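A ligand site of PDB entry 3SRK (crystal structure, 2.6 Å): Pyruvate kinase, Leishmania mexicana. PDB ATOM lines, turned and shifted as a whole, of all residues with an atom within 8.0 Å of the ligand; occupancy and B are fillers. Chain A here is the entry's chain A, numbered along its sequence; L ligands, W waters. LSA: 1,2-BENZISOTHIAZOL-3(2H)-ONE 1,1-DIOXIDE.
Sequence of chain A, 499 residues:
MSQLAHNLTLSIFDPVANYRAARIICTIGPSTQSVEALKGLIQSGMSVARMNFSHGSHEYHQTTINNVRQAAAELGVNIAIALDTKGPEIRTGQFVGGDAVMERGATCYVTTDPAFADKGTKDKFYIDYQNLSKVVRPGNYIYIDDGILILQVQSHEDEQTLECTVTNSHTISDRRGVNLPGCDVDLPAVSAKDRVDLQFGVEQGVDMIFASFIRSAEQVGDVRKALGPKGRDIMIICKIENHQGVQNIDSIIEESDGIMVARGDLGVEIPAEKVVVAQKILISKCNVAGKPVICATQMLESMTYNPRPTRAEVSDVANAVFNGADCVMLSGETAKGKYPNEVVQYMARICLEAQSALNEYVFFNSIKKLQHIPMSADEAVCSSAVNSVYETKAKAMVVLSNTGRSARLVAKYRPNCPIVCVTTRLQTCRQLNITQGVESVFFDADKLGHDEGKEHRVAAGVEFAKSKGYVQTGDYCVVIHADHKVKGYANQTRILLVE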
ATOM      1  N   THR A  27     -12.409 -29.893  -9.659  1.00  0.00           N
ATOM      2  CA  THR A  27     -11.802 -29.290  -8.477  1.00  0.00           C
ATOM      3  C   THR A  27     -10.503 -30.019  -8.150  1.00  0.00           C
ATOM      4  O   THR A  27     -10.465 -31.253  -8.109  1.00  0.00           O
ATOM      5  CB  THR A  27     -12.747 -29.319  -7.252  1.00  0.00           C
ATOM      6  OG1 THR A  27     -13.992 -28.693  -7.601  1.00  0.00           O
ATOM      7  CG2 THR A  27     -12.145 -28.561  -6.073  1.00  0.00           C
ATOM      8  N   ILE A  28      -9.432 -29.259  -7.949  1.00  0.00           N
ATOM      9  CA  ILE A  28      -8.106 -29.829  -7.704  1.00  0.00           C
ATOM     10  C   ILE A  28      -7.852 -29.960  -6.203  1.00  0.00           C
ATOM     11  O   ILE A  28      -7.939 -28.985  -5.455  1.00  0.00           O
ATOM     12  CB  ILE A  28      -6.968 -29.000  -8.374  1.00  0.00           C
ATOM     13  CG1 ILE A  28      -7.320 -28.622  -9.834  1.00  0.00           C
ATOM     14  CG2 ILE A  28      -5.626 -29.731  -8.280  1.00  0.00           C
ATOM     15  CD1 ILE A  28      -7.639 -29.798 -10.769  1.00  0.00           C
ATOM     16  N   GLY A  29      -7.543 -31.187  -5.773  1.00  0.00           N
ATOM     17  CA  GLY A  29      -7.239 -31.473  -4.375  1.00  0.00           C
ATOM     18  C   GLY A  29      -6.079 -32.431  -4.226  1.00  0.00           C
ATOM     19  O   GLY A  29      -5.262 -32.574  -5.145  1.00  0.00           O
ATOM     20  N   PRO A  30      -5.984 -33.103  -3.063  1.00  0.00           N
ATOM     21  CA  PRO A  30      -4.896 -34.047  -2.752  1.00  0.00           C
ATOM     22  C   PRO A  30      -4.675 -35.108  -3.835  1.00  0.00           C
ATOM     23  O   PRO A  30      -3.531 -35.483  -4.086  1.00  0.00           O
ATOM     24  CB  PRO A  30      -5.375 -34.707  -1.447  1.00  0.00           C
ATOM     25  CG  PRO A  30      -6.196 -33.650  -0.789  1.00  0.00           C
ATOM     26  CD  PRO A  30      -6.891 -32.924  -1.916  1.00  0.00           C
ATOM     27  N   SER A  31      -5.746 -35.553  -4.466  1.00  0.00           N
ATOM     28  CA  SER A  31      -5.679 -36.608  -5.475  1.00  0.00           C
ATOM     29  C   SER A  31      -5.195 -36.134  -6.838  1.00  0.00           C
ATOM     30  O   SER A  31      -4.816 -36.948  -7.680  1.00  0.00           O
ATOM     31  CB  SER A  31      -7.045 -37.287  -5.628  1.00  0.00           C
ATOM     32  OG  SER A  31      -7.507 -37.799  -4.392  1.00  0.00           O
ATOM     33  N   THR A  32      -5.206 -34.815  -7.061  1.00  0.00           N
ATOM     34  CA  THR A  32      -4.994 -34.281  -8.408  1.00  0.00           C
ATOM     35  C   THR A  32      -3.975 -33.147  -8.578  1.00  0.00           C
ATOM     36  O   THR A  32      -3.761 -32.675  -9.699  1.00  0.00           O
ATOM     37  CB  THR A  32      -6.333 -33.840  -9.062  1.00  0.00           C
ATOM     38  OG1 THR A  32      -7.212 -33.312  -8.057  1.00  0.00           O
ATOM     39  CG2 THR A  32      -6.990 -35.015  -9.759  1.00  0.00           C
ATOM     40  N   GLN A  33      -3.341 -32.722  -7.491  1.00  0.00           N
ATOM     41  CA  GLN A  33      -2.461 -31.541  -7.553  1.00  0.00           C
ATOM     42  C   GLN A  33      -1.178 -31.729  -8.384  1.00  0.00           C
ATOM     43  O   GLN A  33      -0.740 -30.790  -9.044  1.00  0.00           O
ATOM     44  CB  GLN A  33      -2.126 -31.020  -6.143  1.00  0.00           C
ATOM     45  CG  GLN A  33      -1.580 -29.586  -6.155  1.00  0.00           C
ATOM     46  CD  GLN A  33      -1.386 -29.013  -4.759  1.00  0.00           C
ATOM     47  OE1 GLN A  33      -0.648 -29.559  -3.950  1.00  0.00           O
ATOM     48  NE2 GLN A  33      -2.049 -27.890  -4.495  1.00  0.00           N
ATOM     49  N   ARG A  50     -10.627 -25.790 -10.859  1.00  0.00           N
ATOM     50  CA  ARG A  50     -11.259 -25.055  -9.756  1.00  0.00           C
ATOM     51  C   ARG A  50     -10.438 -25.154  -8.472  1.00  0.00           C
ATOM     52  O   ARG A  50     -10.068 -26.251  -8.048  1.00  0.00           O
ATOM     53  CB  ARG A  50     -12.673 -25.582  -9.509  1.00  0.00           C
ATOM     54  CG  ARG A  50     -13.367 -24.976  -8.289  1.00  0.00           C
ATOM     55  CD  ARG A  50     -14.759 -25.561  -8.111  1.00  0.00           C
ATOM     56  NE  ARG A  50     -15.448 -25.001  -6.945  1.00  0.00           N
ATOM     57  CZ  ARG A  50     -15.532 -25.594  -5.756  1.00  0.00           C
ATOM     58  NH1 ARG A  50     -14.962 -26.780  -5.554  1.00  0.00           N
ATOM     59  NH2 ARG A  50     -16.173 -24.999  -4.771  1.00  0.00           N
ATOM     60  N   MET A  51     -10.159 -23.995  -7.881  1.00  0.00           N
ATOM     61  CA  MET A  51      -9.487 -23.943  -6.590  1.00  0.00           C
ATOM     62  C   MET A  51     -10.497 -23.554  -5.518  1.00  0.00           C
ATOM     63  O   MET A  51     -11.083 -22.464  -5.586  1.00  0.00           O
ATOM     64  CB  MET A  51      -8.345 -22.920  -6.610  1.00  0.00           C
ATOM     65  CG  MET A  51      -7.312 -23.133  -7.705  1.00  0.00           C
ATOM     66  SD  MET A  51      -6.026 -21.864  -7.699  1.00  0.00           S
ATOM     67  CE  MET A  51      -6.969 -20.373  -7.989  1.00  0.00           C
ATOM     68  N   ASN A  52     -10.702 -24.441  -4.552  1.00  0.00           N
ATOM     69  CA  ASN A  52     -11.614 -24.180  -3.443  1.00  0.00           C
ATOM     70  C   ASN A  52     -10.906 -23.495  -2.279  1.00  0.00           C
ATOM     71  O   ASN A  52     -10.079 -24.104  -1.599  1.00  0.00           O
ATOM     72  CB  ASN A  52     -12.300 -25.473  -2.972  1.00  0.00           C
ATOM     73  CG  ASN A  52     -13.443 -25.218  -2.001  1.00  0.00           C
ATOM     74  OD1 ASN A  52     -13.825 -24.068  -1.746  1.00  0.00           O
ATOM     75  ND2 ASN A  52     -14.002 -26.287  -1.462  1.00  0.00           N
ATOM     76  N   PHE A  53     -11.250 -22.232  -2.062  1.00  0.00           N
ATOM     77  CA  PHE A  53     -10.658 -21.436  -0.996  1.00  0.00           C
ATOM     78  C   PHE A  53     -11.462 -21.487   0.302  1.00  0.00           C
ATOM     79  O   PHE A  53     -11.349 -20.601   1.154  1.00  0.00           O
ATOM     80  CB  PHE A  53     -10.414 -20.001  -1.462  1.00  0.00           C
ATOM     81  CG  PHE A  53      -9.124 -19.816  -2.211  1.00  0.00           C
ATOM     82  CD1 PHE A  53      -8.938 -20.387  -3.466  1.00  0.00           C
ATOM     83  CD2 PHE A  53      -8.080 -19.079  -1.646  1.00  0.00           C
ATOM     84  CE1 PHE A  53      -7.739 -20.220  -4.163  1.00  0.00           C
ATOM     85  CE2 PHE A  53      -6.882 -18.904  -2.337  1.00  0.00           C
ATOM     86  CZ  PHE A  53      -6.705 -19.473  -3.596  1.00  0.00           C
ATOM     87  N   SER A  54     -12.271 -22.532   0.450  1.00  0.00           N
ATOM     88  CA  SER A  54     -12.844 -22.896   1.751  1.00  0.00           C
ATOM     89  C   SER A  54     -11.763 -23.594   2.563  1.00  0.00           C
ATOM     90  O   SER A  54     -11.757 -23.507   3.788  1.00  0.00           O
ATOM     91  CB  SER A  54     -14.050 -23.823   1.589  1.00  0.00           C
ATOM     92  OG  SER A  54     -15.177 -23.137   1.074  1.00  0.00           O
ATOM     93  N   HIS A  55     -10.868 -24.282   1.862  1.00  0.00           N
ATOM     94  CA  HIS A  55      -9.769 -25.040   2.460  1.00  0.00           C
ATOM     95  C   HIS A  55      -8.435 -24.579   1.873  1.00  0.00           C
ATOM     96  O   HIS A  55      -8.408 -23.834   0.888  1.00  0.00           O
ATOM     97  CB  HIS A  55      -9.952 -26.534   2.200  1.00  0.00           C
ATOM     98  CG  HIS A  55     -11.288 -27.072   2.622  1.00  0.00           C
ATOM     99  ND1 HIS A  55     -12.409 -26.993   1.821  1.00  0.00           N
ATOM    100  CD2 HIS A  55     -11.687 -27.706   3.749  1.00  0.00           C
ATOM    101  CE1 HIS A  55     -13.436 -27.538   2.446  1.00  0.00           C
ATOM    102  NE2 HIS A  55     -13.017 -27.983   3.616  1.00  0.00           N
ATOM    103  N   GLY A  56      -7.338 -25.021   2.479  1.00  0.00           N
ATOM    104  CA  GLY A  56      -5.991 -24.803   1.943  1.00  0.00           C
ATOM    105  C   GLY A  56      -5.441 -23.390   2.088  1.00  0.00           C
ATOM    106  O   GLY A  56      -6.188 -22.429   2.215  1.00  0.00           O
ATOM    107  N   SER A  57      -4.112 -23.290   2.072  1.00  0.00           N
ATOM    108  CA  SER A  57      -3.425 -22.009   2.201  1.00  0.00           C
ATOM    109  C   SER A  57      -2.990 -21.463   0.835  1.00  0.00           C
ATOM    110  O   SER A  57      -3.130 -22.139  -0.191  1.00  0.00           O
ATOM    111  CB  SER A  57      -2.216 -22.139   3.117  1.00  0.00           C
ATOM    112  OG  SER A  57      -1.161 -22.841   2.482  1.00  0.00           O
ATOM    113  N   TYR A  60      -0.402 -23.590  -0.836  1.00  0.00           N
ATOM    114  CA  TYR A  60      -1.025 -24.801  -1.399  1.00  0.00           C
ATOM    115  C   TYR A  60      -1.657 -24.535  -2.758  1.00  0.00           C
ATOM    116  O   TYR A  60      -1.422 -25.283  -3.714  1.00  0.00           O
ATOM    117  CB  TYR A  60      -2.065 -25.380  -0.440  1.00  0.00           C
ATOM    118  CG  TYR A  60      -2.815 -26.557  -1.008  1.00  0.00           C
ATOM    119  CD1 TYR A  60      -2.287 -27.850  -0.953  1.00  0.00           C
ATOM    120  CD2 TYR A  60      -4.061 -26.389  -1.621  1.00  0.00           C
ATOM    121  CE1 TYR A  60      -2.967 -28.935  -1.476  1.00  0.00           C
ATOM    122  CE2 TYR A  60      -4.757 -27.477  -2.159  1.00  0.00           C
ATOM    123  CZ  TYR A  60      -4.202 -28.748  -2.079  1.00  0.00           C
ATOM    124  OH  TYR A  60      -4.879 -29.819  -2.602  1.00  0.00           O
ATOM    125  N   HIS A  61      -2.451 -23.478  -2.845  1.00  0.00           N
ATOM    126  CA  HIS A  61      -3.113 -23.107  -4.099  1.00  0.00           C
ATOM    127  C   HIS A  61      -2.126 -22.551  -5.121  1.00  0.00           C
ATOM    128  O   HIS A  61      -2.377 -22.592  -6.323  1.00  0.00           O
ATOM    129  CB  HIS A  61      -4.251 -22.111  -3.837  1.00  0.00           C
ATOM    130  CG  HIS A  61      -5.371 -22.685  -3.031  1.00  0.00           C
ATOM    131  ND1 HIS A  61      -6.157 -23.725  -3.486  1.00  0.00           N
ATOM    132  CD2 HIS A  61      -5.837 -22.375  -1.795  1.00  0.00           C
ATOM    133  CE1 HIS A  61      -7.065 -24.019  -2.569  1.00  0.00           C
ATOM    134  NE2 HIS A  61      -6.894 -23.212  -1.539  1.00  0.00           N
ATOM    135  N   THR A  64      -0.924 -25.413  -7.089  1.00  0.00           N
ATOM    136  CA  THR A  64      -2.005 -25.721  -8.026  1.00  0.00           C
ATOM    137  C   THR A  64      -1.896 -24.827  -9.265  1.00  0.00           C
ATOM    138  O   THR A  64      -1.854 -25.320 -10.387  1.00  0.00           O
ATOM    139  CB  THR A  64      -3.412 -25.525  -7.393  1.00  0.00           C
ATOM    140  OG1 THR A  64      -3.460 -26.193  -6.134  1.00  0.00           O
ATOM    141  CG2 THR A  64      -4.498 -26.080  -8.310  1.00  0.00           C
ATOM    142  N   SER A 331     -16.595 -31.725  -7.777  1.00  0.00           N
ATOM    143  CA  SER A 331     -16.020 -31.244  -6.528  1.00  0.00           C
ATOM    144  C   SER A 331     -15.087 -32.286  -5.913  1.00  0.00           C
ATOM    145  O   SER A 331     -13.931 -32.433  -6.336  1.00  0.00           O
ATOM    146  CB  SER A 331     -17.116 -30.825  -5.543  1.00  0.00           C
ATOM    147  OG  SER A 331     -17.753 -29.633  -5.963  1.00  0.00           O
ATOM    148  N   GLY A 332     -15.592 -33.032  -4.926  1.00  0.00           N
ATOM    149  CA  GLY A 332     -14.805 -34.049  -4.243  1.00  0.00           C
ATOM    150  C   GLY A 332     -14.295 -35.164  -5.150  1.00  0.00           C
ATOM    151  O   GLY A 332     -13.252 -35.758  -4.867  1.00  0.00           O
ATOM    152  N   THR A 334     -12.866 -35.223  -8.033  1.00  0.00           N
ATOM    153  CA  THR A 334     -11.521 -34.998  -8.563  1.00  0.00           C
ATOM    154  C   THR A 334     -10.578 -34.488  -7.487  1.00  0.00           C
ATOM    155  O   THR A 334      -9.370 -34.694  -7.580  1.00  0.00           O
ATOM    156  CB  THR A 334     -11.530 -34.027  -9.760  1.00  0.00           C
ATOM    157  OG1 THR A 334     -12.169 -32.798  -9.381  1.00  0.00           O
ATOM    158  CG2 THR A 334     -12.268 -34.638 -10.942  1.00  0.00           C
ATOM    159  N   ALA A 335     -11.123 -33.823  -6.472  1.00  0.00           N
ATOM    160  CA  ALA A 335     -10.316 -33.290  -5.372  1.00  0.00           C
ATOM    161  C   ALA A 335      -9.828 -34.382  -4.428  1.00  0.00           C
ATOM    162  O   ALA A 335      -8.627 -34.574  -4.264  1.00  0.00           O
ATOM    163  CB  ALA A 335     -11.089 -32.223  -4.604  1.00  0.00           C
ATOM    164  N   LYS A 336     -10.790 -35.113  -3.798  1.00  0.00           N
ATOM    165  CA  LYS A 336     -10.474 -36.097  -2.765  1.00  0.00           C
ATOM    166  C   LYS A 336     -10.802 -37.533  -3.226  1.00  0.00           C
ATOM    167  O   LYS A 336     -10.648 -38.485  -2.461  1.00  0.00           O
ATOM    168  CB  LYS A 336     -11.264 -35.742  -1.490  1.00  0.00           C
ATOM    169  CG  LYS A 336     -10.829 -34.399  -0.906  1.00  0.00           C
ATOM    170  CD  LYS A 336     -11.726 -33.951   0.246  1.00  0.00           C
ATOM    171  CE  LYS A 336     -11.038 -32.869   1.100  1.00  0.00           C
ATOM    172  NZ  LYS A 336     -11.369 -31.535   0.547  1.00  0.00           N
HETATM  173  C4  LSA L   1      -6.432 -30.002   1.261  1.00  0.00           C
HETATM  174  C5  LSA L   1      -7.119 -29.334   0.243  1.00  0.00           C
HETATM  175  C6  LSA L   1      -8.474 -29.570   0.068  1.00  0.00           C
HETATM  176  C7  LSA L   1     -10.535 -30.489   0.483  1.00  0.00           C
HETATM  177  C3  LSA L   1      -7.111 -30.895   2.088  1.00  0.00           C
HETATM  178  S10 LSA L   1      -9.683 -28.966  -1.008  1.00  0.00           S
HETATM  179  N9  LSA L   1     -10.944 -29.339  -0.080  1.00  0.00           N
HETATM  180  C1  LSA L   1      -9.176 -30.456   0.898  1.00  0.00           C
HETATM  181  C2  LSA L   1      -8.484 -31.117   1.910  1.00  0.00           C
HETATM  182  O12 LSA L   1      -9.509 -27.485  -1.236  1.00  0.00           O
HETATM  183  O11 LSA L   1      -9.695 -29.712  -2.327  1.00  0.00           O
HETATM  184  O   HOH W   1     -13.275 -31.029  -1.426  1.00  0.00           O
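A carbon (C7) of the ligand is bonded to the side-chain amino group (NZ) of Lys 336 (1.3 Å). N9 of the ligand is in hydrogen-bond range of ND1 of His 55 (3.4 Å).
O of Asn 52 lies close to O12 of the ligand, 3.4 Å away. Merely in contact with the ligand: Ile 28, Gly 29, Tyr 60 and Ala 335. Hydrophobic or aromatic side chains within 4 Å of the ligand: His 55, Tyr 60 and Ala 335. Seven residues have an atom within 4 Å of the ligand: Ile 28, Gly 29, Asn 52, His 55, Tyr 60, Ala 335 and Lys 336.
The backbone carbonyl oxygen (O) of Tyr 60 lies within hydrogen-bond range of the side-chain amide nitrogen (NE2) of Gln 33. O of His 55 sits at hydrogen-bond distance from NE2 of His 61, 2.9 Å away. N of Gly 29 lies within hydrogen-bond range of OG1 of Thr 32 (3.1 Å). O of Asn 52 sits close to NE2 of His 61 (3.3 Å). The backbone NH of Ser 54 is in hydrogen-bond range of the side-chain amide oxygen of Asn 52 (3.1 Å). The backbone NH of Tyr 60 lies within hydrogen-bond range of the side-chain hydroxyl of Ser 57 (3.5 Å). O of Arg 50 is in hydrogen-bond range of N of Ile 28 (3.1 Å). The backbone carbonyl oxygen of Tyr 60 sits at hydrogen-bond distance from the side-chain hydroxyl of Thr 64 (3.3 Å).
Water W1 lies within hydrogen-bond range of NZ of Lys 336 and N9 of the ligand.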
